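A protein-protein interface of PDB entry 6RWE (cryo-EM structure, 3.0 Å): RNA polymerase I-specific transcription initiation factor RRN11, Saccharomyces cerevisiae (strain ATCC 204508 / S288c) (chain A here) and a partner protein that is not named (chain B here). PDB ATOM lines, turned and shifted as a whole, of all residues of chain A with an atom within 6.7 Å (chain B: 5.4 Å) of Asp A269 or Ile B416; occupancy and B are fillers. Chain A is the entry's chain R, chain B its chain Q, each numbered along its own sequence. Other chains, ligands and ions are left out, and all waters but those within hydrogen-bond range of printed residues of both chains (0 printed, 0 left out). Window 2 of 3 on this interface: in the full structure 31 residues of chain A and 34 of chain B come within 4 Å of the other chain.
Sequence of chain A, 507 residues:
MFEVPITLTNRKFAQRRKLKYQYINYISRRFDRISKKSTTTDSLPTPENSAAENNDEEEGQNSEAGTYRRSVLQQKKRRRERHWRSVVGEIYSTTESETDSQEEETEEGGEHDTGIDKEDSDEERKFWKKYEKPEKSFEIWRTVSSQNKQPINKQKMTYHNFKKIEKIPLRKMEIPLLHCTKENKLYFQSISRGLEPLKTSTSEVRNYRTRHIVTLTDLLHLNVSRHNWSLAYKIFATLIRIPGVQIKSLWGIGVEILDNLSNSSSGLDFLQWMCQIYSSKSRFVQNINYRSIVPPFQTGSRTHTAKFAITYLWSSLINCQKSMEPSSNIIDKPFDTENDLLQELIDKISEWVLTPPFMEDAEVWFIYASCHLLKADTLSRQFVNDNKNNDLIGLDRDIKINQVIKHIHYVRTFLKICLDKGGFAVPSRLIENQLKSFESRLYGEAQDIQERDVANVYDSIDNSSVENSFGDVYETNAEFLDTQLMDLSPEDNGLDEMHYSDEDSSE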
ATOM      1  N   TYR A 233      33.260  17.647 -21.664  1.00  0.00           N
ATOM      2  CA  TYR A 233      32.480  18.807 -21.261  1.00  0.00           C
ATOM      3  C   TYR A 233      32.796  20.013 -22.127  1.00  0.00           C
ATOM      4  O   TYR A 233      31.903  20.813 -22.417  1.00  0.00           O
ATOM      5  CB  TYR A 233      32.744  19.133 -19.796  1.00  0.00           C
ATOM      6  CG  TYR A 233      32.043  20.374 -19.305  1.00  0.00           C
ATOM      7  CD1 TYR A 233      30.688  20.368 -19.037  1.00  0.00           C
ATOM      8  CD2 TYR A 233      32.745  21.554 -19.105  1.00  0.00           C
ATOM      9  CE1 TYR A 233      30.052  21.497 -18.586  1.00  0.00           C
ATOM     10  CE2 TYR A 233      32.115  22.688 -18.658  1.00  0.00           C
ATOM     11  CZ  TYR A 233      30.769  22.653 -18.401  1.00  0.00           C
ATOM     12  OH  TYR A 233      30.141  23.785 -17.951  1.00  0.00           O
ATOM     13  N   ILE A 257      27.486  16.009 -16.948  1.00  0.00           N
ATOM     14  CA  ILE A 257      27.336  16.833 -15.765  1.00  0.00           C
ATOM     15  C   ILE A 257      27.265  15.962 -14.522  1.00  0.00           C
ATOM     16  O   ILE A 257      27.828  16.316 -13.483  1.00  0.00           O
ATOM     17  CB  ILE A 257      26.088  17.715 -15.874  1.00  0.00           C
ATOM     18  CG1 ILE A 257      26.050  18.451 -17.195  1.00  0.00           C
ATOM     19  CG2 ILE A 257      26.117  18.793 -14.832  1.00  0.00           C
ATOM     20  CD1 ILE A 257      24.721  19.076 -17.418  1.00  0.00           C
ATOM     21  N   SER A 265      26.884  20.964 -12.336  1.00  0.00           N
ATOM     22  CA  SER A 265      25.548  21.510 -12.147  1.00  0.00           C
ATOM     23  C   SER A 265      24.565  20.456 -11.664  1.00  0.00           C
ATOM     24  O   SER A 265      23.358  20.596 -11.890  1.00  0.00           O
ATOM     25  CB  SER A 265      25.039  22.140 -13.444  1.00  0.00           C
ATOM     26  OG  SER A 265      25.810  23.272 -13.798  1.00  0.00           O
ATOM     27  N   SER A 266      25.075  19.371 -11.072  1.00  0.00           N
ATOM     28  CA  SER A 266      24.393  18.220 -10.480  1.00  0.00           C
ATOM     29  C   SER A 266      23.673  17.351 -11.502  1.00  0.00           C
ATOM     30  O   SER A 266      23.109  16.322 -11.118  1.00  0.00           O
ATOM     31  CB  SER A 266      23.401  18.618  -9.375  1.00  0.00           C
ATOM     32  OG  SER A 266      22.791  17.472  -8.814  1.00  0.00           O
ATOM     33  N   GLY A 267      23.655  17.724 -12.780  1.00  0.00           N
ATOM     34  CA  GLY A 267      23.043  16.926 -13.824  1.00  0.00           C
ATOM     35  C   GLY A 267      21.543  17.084 -13.910  1.00  0.00           C
ATOM     36  O   GLY A 267      20.985  17.272 -14.991  1.00  0.00           O
ATOM     37  N   LEU A 268      20.890  17.027 -12.756  1.00  0.00           N
ATOM     38  CA  LEU A 268      19.447  17.054 -12.642  1.00  0.00           C
ATOM     39  C   LEU A 268      18.847  18.392 -13.045  1.00  0.00           C
ATOM     40  O   LEU A 268      17.692  18.432 -13.478  1.00  0.00           O
ATOM     41  CB  LEU A 268      19.083  16.710 -11.202  1.00  0.00           C
ATOM     42  CG  LEU A 268      17.639  16.466 -10.829  1.00  0.00           C
ATOM     43  CD1 LEU A 268      17.145  15.284 -11.605  1.00  0.00           C
ATOM     44  CD2 LEU A 268      17.587  16.198  -9.354  1.00  0.00           C
ATOM     45  N   ASP A 269      19.599  19.483 -12.928  1.00  0.00           N
ATOM     46  CA  ASP A 269      19.076  20.778 -13.334  1.00  0.00           C
ATOM     47  C   ASP A 269      18.990  20.909 -14.844  1.00  0.00           C
ATOM     48  O   ASP A 269      18.140  21.648 -15.348  1.00  0.00           O
ATOM     49  CB  ASP A 269      19.934  21.903 -12.764  1.00  0.00           C
ATOM     50  CG  ASP A 269      19.723  22.097 -11.282  1.00  0.00           C
ATOM     51  OD1 ASP A 269      18.611  21.810 -10.796  1.00  0.00           O
ATOM     52  OD2 ASP A 269      20.666  22.546 -10.600  1.00  0.00           O
ATOM     53  N   PHE A 270      19.852  20.212 -15.579  1.00  0.00           N
ATOM     54  CA  PHE A 270      19.722  20.212 -17.027  1.00  0.00           C
ATOM     55  C   PHE A 270      18.508  19.423 -17.480  1.00  0.00           C
ATOM     56  O   PHE A 270      17.877  19.779 -18.478  1.00  0.00           O
ATOM     57  CB  PHE A 270      20.981  19.657 -17.675  1.00  0.00           C
ATOM     58  CG  PHE A 270      20.869  19.514 -19.146  1.00  0.00           C
ATOM     59  CD1 PHE A 270      20.752  20.625 -19.948  1.00  0.00           C
ATOM     60  CD2 PHE A 270      20.880  18.273 -19.730  1.00  0.00           C
ATOM     61  CE1 PHE A 270      20.643  20.494 -21.308  1.00  0.00           C
ATOM     62  CE2 PHE A 270      20.777  18.139 -21.085  1.00  0.00           C
ATOM     63  CZ  PHE A 270      20.656  19.249 -21.875  1.00  0.00           C
ATOM     64  N   LEU A 271      18.165  18.359 -16.758  1.00  0.00           N
ATOM     65  CA  LEU A 271      16.973  17.596 -17.094  1.00  0.00           C
ATOM     66  C   LEU A 271      15.715  18.392 -16.811  1.00  0.00           C
ATOM     67  O   LEU A 271      14.718  18.240 -17.522  1.00  0.00           O
ATOM     68  CB  LEU A 271      16.953  16.278 -16.323  1.00  0.00           C
ATOM     69  CG  LEU A 271      17.706  15.064 -16.872  1.00  0.00           C
ATOM     70  CD1 LEU A 271      19.199  15.197 -16.804  1.00  0.00           C
ATOM     71  CD2 LEU A 271      17.310  13.869 -16.088  1.00  0.00           C
ATOM     72  N   GLN A 272      15.748  19.248 -15.789  1.00  0.00           N
ATOM     73  CA  GLN A 272      14.631  20.149 -15.541  1.00  0.00           C
ATOM     74  C   GLN A 272      14.497  21.171 -16.655  1.00  0.00           C
ATOM     75  O   GLN A 272      13.376  21.532 -17.021  1.00  0.00           O
ATOM     76  CB  GLN A 272      14.803  20.850 -14.197  1.00  0.00           C
ATOM     77  CG  GLN A 272      13.608  21.671 -13.769  1.00  0.00           C
ATOM     78  CD  GLN A 272      13.817  22.346 -12.437  1.00  0.00           C
ATOM     79  OE1 GLN A 272      14.881  22.235 -11.834  1.00  0.00           O
ATOM     80  NE2 GLN A 272      12.801  23.055 -11.968  1.00  0.00           N
ATOM     81  N   TRP A 273      15.621  21.615 -17.225  1.00  0.00           N
ATOM     82  CA  TRP A 273      15.585  22.539 -18.352  1.00  0.00           C
ATOM     83  C   TRP A 273      14.914  21.914 -19.565  1.00  0.00           C
ATOM     84  O   TRP A 273      14.188  22.595 -20.297  1.00  0.00           O
ATOM     85  CB  TRP A 273      17.000  22.959 -18.729  1.00  0.00           C
ATOM     86  CG  TRP A 273      17.048  23.995 -19.789  1.00  0.00           C
ATOM     87  CD1 TRP A 273      16.922  25.331 -19.621  1.00  0.00           C
ATOM     88  CD2 TRP A 273      17.128  23.775 -21.199  1.00  0.00           C
ATOM     89  NE1 TRP A 273      16.982  25.969 -20.830  1.00  0.00           N
ATOM     90  CE2 TRP A 273      17.096  25.029 -21.817  1.00  0.00           C
ATOM     91  CE3 TRP A 273      17.244  22.639 -21.994  1.00  0.00           C
ATOM     92  CZ2 TRP A 273      17.183  25.182 -23.188  1.00  0.00           C
ATOM     93  CZ3 TRP A 273      17.321  22.791 -23.350  1.00  0.00           C
ATOM     94  CH2 TRP A 273      17.290  24.049 -23.937  1.00  0.00           C
ATOM     95  N   MET A 274      15.164  20.625 -19.805  1.00  0.00           N
ATOM     96  CA  MET A 274      14.612  19.951 -20.975  1.00  0.00           C
ATOM     97  C   MET A 274      13.103  19.815 -20.868  1.00  0.00           C
ATOM     98  O   MET A 274      12.375  20.095 -21.823  1.00  0.00           O
ATOM     99  CB  MET A 274      15.244  18.573 -21.136  1.00  0.00           C
ATOM    100  CG  MET A 274      16.674  18.571 -21.595  1.00  0.00           C
ATOM    101  SD  MET A 274      16.816  19.253 -23.245  1.00  0.00           S
ATOM    102  CE  MET A 274      15.915  18.025 -24.164  1.00  0.00           C
ATOM    103  N   TYR A 312      14.004  12.481 -15.657  1.00  0.00           N
ATOM    104  CA  TYR A 312      13.955  13.494 -14.610  1.00  0.00           C
ATOM    105  C   TYR A 312      13.248  12.978 -13.373  1.00  0.00           C
ATOM    106  O   TYR A 312      13.545  13.403 -12.256  1.00  0.00           O
ATOM    107  CB  TYR A 312      13.265  14.745 -15.126  1.00  0.00           C
ATOM    108  CG  TYR A 312      13.204  15.847 -14.116  1.00  0.00           C
ATOM    109  CD1 TYR A 312      14.344  16.536 -13.757  1.00  0.00           C
ATOM    110  CD2 TYR A 312      12.009  16.209 -13.529  1.00  0.00           C
ATOM    111  CE1 TYR A 312      14.297  17.546 -12.835  1.00  0.00           C
ATOM    112  CE2 TYR A 312      11.953  17.222 -12.611  1.00  0.00           C
ATOM    113  CZ  TYR A 312      13.099  17.886 -12.267  1.00  0.00           C
ATOM    114  OH  TYR A 312      13.048  18.902 -11.349  1.00  0.00           O
ATOM    115  N   LYS B 412      19.356  30.685 -20.312  1.00  0.00           N
ATOM    116  CA  LYS B 412      19.334  29.839 -19.132  1.00  0.00           C
ATOM    117  C   LYS B 412      20.229  28.626 -19.321  1.00  0.00           C
ATOM    118  O   LYS B 412      20.906  28.192 -18.385  1.00  0.00           O
ATOM    119  CB  LYS B 412      17.895  29.427 -18.857  1.00  0.00           C
ATOM    120  CG  LYS B 412      17.640  28.746 -17.551  1.00  0.00           C
ATOM    121  CD  LYS B 412      16.163  28.434 -17.464  1.00  0.00           C
ATOM    122  CE  LYS B 412      15.364  29.714 -17.298  1.00  0.00           C
ATOM    123  NZ  LYS B 412      13.915  29.444 -17.151  1.00  0.00           N
ATOM    124  N   LEU B 413      20.250  28.078 -20.532  1.00  0.00           N
ATOM    125  CA  LEU B 413      21.101  26.934 -20.824  1.00  0.00           C
ATOM    126  C   LEU B 413      22.568  27.324 -20.922  1.00  0.00           C
ATOM    127  O   LEU B 413      23.440  26.550 -20.522  1.00  0.00           O
ATOM    128  CB  LEU B 413      20.606  26.247 -22.094  1.00  0.00           C
ATOM    129  CG  LEU B 413      21.495  25.185 -22.722  1.00  0.00           C
ATOM    130  CD1 LEU B 413      20.727  23.964 -23.019  1.00  0.00           C
ATOM    131  CD2 LEU B 413      21.986  25.723 -24.032  1.00  0.00           C
ATOM    132  N   TYR B 414      22.868  28.523 -21.398  1.00  0.00           N
ATOM    133  CA  TYR B 414      24.257  28.946 -21.409  1.00  0.00           C
ATOM    134  C   TYR B 414      24.766  29.276 -20.018  1.00  0.00           C
ATOM    135  O   TYR B 414      25.981  29.320 -19.815  1.00  0.00           O
ATOM    136  CB  TYR B 414      24.448  30.142 -22.335  1.00  0.00           C
ATOM    137  CG  TYR B 414      24.266  29.822 -23.800  1.00  0.00           C
ATOM    138  CD1 TYR B 414      24.313  28.522 -24.256  1.00  0.00           C
ATOM    139  CD2 TYR B 414      24.026  30.824 -24.721  1.00  0.00           C
ATOM    140  CE1 TYR B 414      24.136  28.225 -25.578  1.00  0.00           C
ATOM    141  CE2 TYR B 414      23.851  30.532 -26.053  1.00  0.00           C
ATOM    142  CZ  TYR B 414      23.910  29.229 -26.470  1.00  0.00           C
ATOM    143  OH  TYR B 414      23.737  28.925 -27.791  1.00  0.00           O
ATOM    144  N   LYS B 415      23.869  29.494 -19.060  1.00  0.00           N
ATOM    145  CA  LYS B 415      24.265  29.544 -17.660  1.00  0.00           C
ATOM    146  C   LYS B 415      24.589  28.155 -17.134  1.00  0.00           C
ATOM    147  O   LYS B 415      25.540  27.984 -16.367  1.00  0.00           O
ATOM    148  CB  LYS B 415      23.157  30.187 -16.830  1.00  0.00           C
ATOM    149  CG  LYS B 415      23.455  30.276 -15.353  1.00  0.00           C
ATOM    150  CD  LYS B 415      24.603  31.230 -15.088  1.00  0.00           C
ATOM    151  CE  LYS B 415      24.859  31.389 -13.600  1.00  0.00           C
ATOM    152  NZ  LYS B 415      26.025  32.271 -13.337  1.00  0.00           N
ATOM    153  N   ILE B 416      23.827  27.146 -17.551  1.00  0.00           N
ATOM    154  CA  ILE B 416      24.059  25.810 -17.020  1.00  0.00           C
ATOM    155  C   ILE B 416      25.189  25.114 -17.764  1.00  0.00           C
ATOM    156  O   ILE B 416      25.750  24.139 -17.256  1.00  0.00           O
ATOM    157  CB  ILE B 416      22.749  25.003 -17.046  1.00  0.00           C
ATOM    158  CG1 ILE B 416      22.774  23.904 -16.007  1.00  0.00           C
ATOM    159  CG2 ILE B 416      22.533  24.320 -18.356  1.00  0.00           C
ATOM    160  CD1 ILE B 416      21.434  23.323 -15.800  1.00  0.00           C
ATOM    161  N   PHE B 417      25.563  25.613 -18.944  1.00  0.00           N
ATOM    162  CA  PHE B 417      26.780  25.216 -19.645  1.00  0.00           C
ATOM    163  C   PHE B 417      27.608  26.463 -19.919  1.00  0.00           C
ATOM    164  O   PHE B 417      27.580  26.989 -21.041  1.00  0.00           O
ATOM    165  CB  PHE B 417      26.484  24.517 -20.968  1.00  0.00           C
ATOM    166  CG  PHE B 417      25.923  23.147 -20.825  1.00  0.00           C
ATOM    167  CD1 PHE B 417      26.751  22.069 -20.594  1.00  0.00           C
ATOM    168  CD2 PHE B 417      24.570  22.930 -20.954  1.00  0.00           C
ATOM    169  CE1 PHE B 417      26.235  20.805 -20.473  1.00  0.00           C
ATOM    170  CE2 PHE B 417      24.051  21.670 -20.830  1.00  0.00           C
ATOM    171  CZ  PHE B 417      24.884  20.611 -20.594  1.00  0.00           C
ATOM    172  N   PRO B 418      28.341  26.972 -18.931  1.00  0.00           N
ATOM    173  CA  PRO B 418      29.266  28.071 -19.218  1.00  0.00           C
ATOM    174  C   PRO B 418      30.390  27.597 -20.120  1.00  0.00           C
ATOM    175  O   PRO B 418      30.917  26.494 -19.957  1.00  0.00           O
ATOM    176  CB  PRO B 418      29.773  28.479 -17.834  1.00  0.00           C
ATOM    177  CG  PRO B 418      29.604  27.269 -17.008  1.00  0.00           C
ATOM    178  CD  PRO B 418      28.383  26.586 -17.511  1.00  0.00           C
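The side-chain hydroxyl (OH) of Tyr A233 sits close to the backbone carbonyl oxygen (O) of Pro B418, at 3.5 Å.
Among the printed residues, pairs that only touch across the chains: Phe A270 with Ile B416 (3.5 Å), Ile A257 with Phe B417 (3.5 Å), Trp A273 with Leu B413 (3.6 Å), Ser A265 with Ile B416 (3.6 Å), Asp A269 with Ile B416 (3.6 Å), Phe A270 with Phe B417 (3.6 Å), Trp A273 with Lys B412 (3.9 Å), Phe A270 with Leu B413 (3.9 Å) and Tyr A233 with Phe B417 (3.9 Å).
Asp A269 touches just one residue of chain B: Ile B416. Of the printed residues of chain B, Trp A273 touches Lys B412 and Leu B413. Lys B415 touches none of the printed residues of chain A. Ile B416 touches just these residues of chain A: Ser A265, Asp A269 and Phe A270. Of the printed residues of chain A, Phe B417 touches Tyr A233 (3.9 Å), Ile A257 (3.5 Å) and Phe A270 (3.6 Å). Printed residues of chain A within 4 Å of Pro B418: Tyr A233 (3.3 Å).
Printed residues of chain B that touch a printed residue of chain A: Lys B412, Leu B413, Ile B416, Phe B417 and Pro B418. Hydrophobic or aromatic side chains of chain B that line the printed part of chain A: Leu B413, Ile B416, Phe B417 and Pro B418. Of the 13 printed residues of chain A, 6 touch a printed residue of chain B. Hydrophobic or aromatic side chains of chain A within 4 Å of the printed part of chain B: Tyr A233, Ile A257, Phe A270 and Trp A273.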
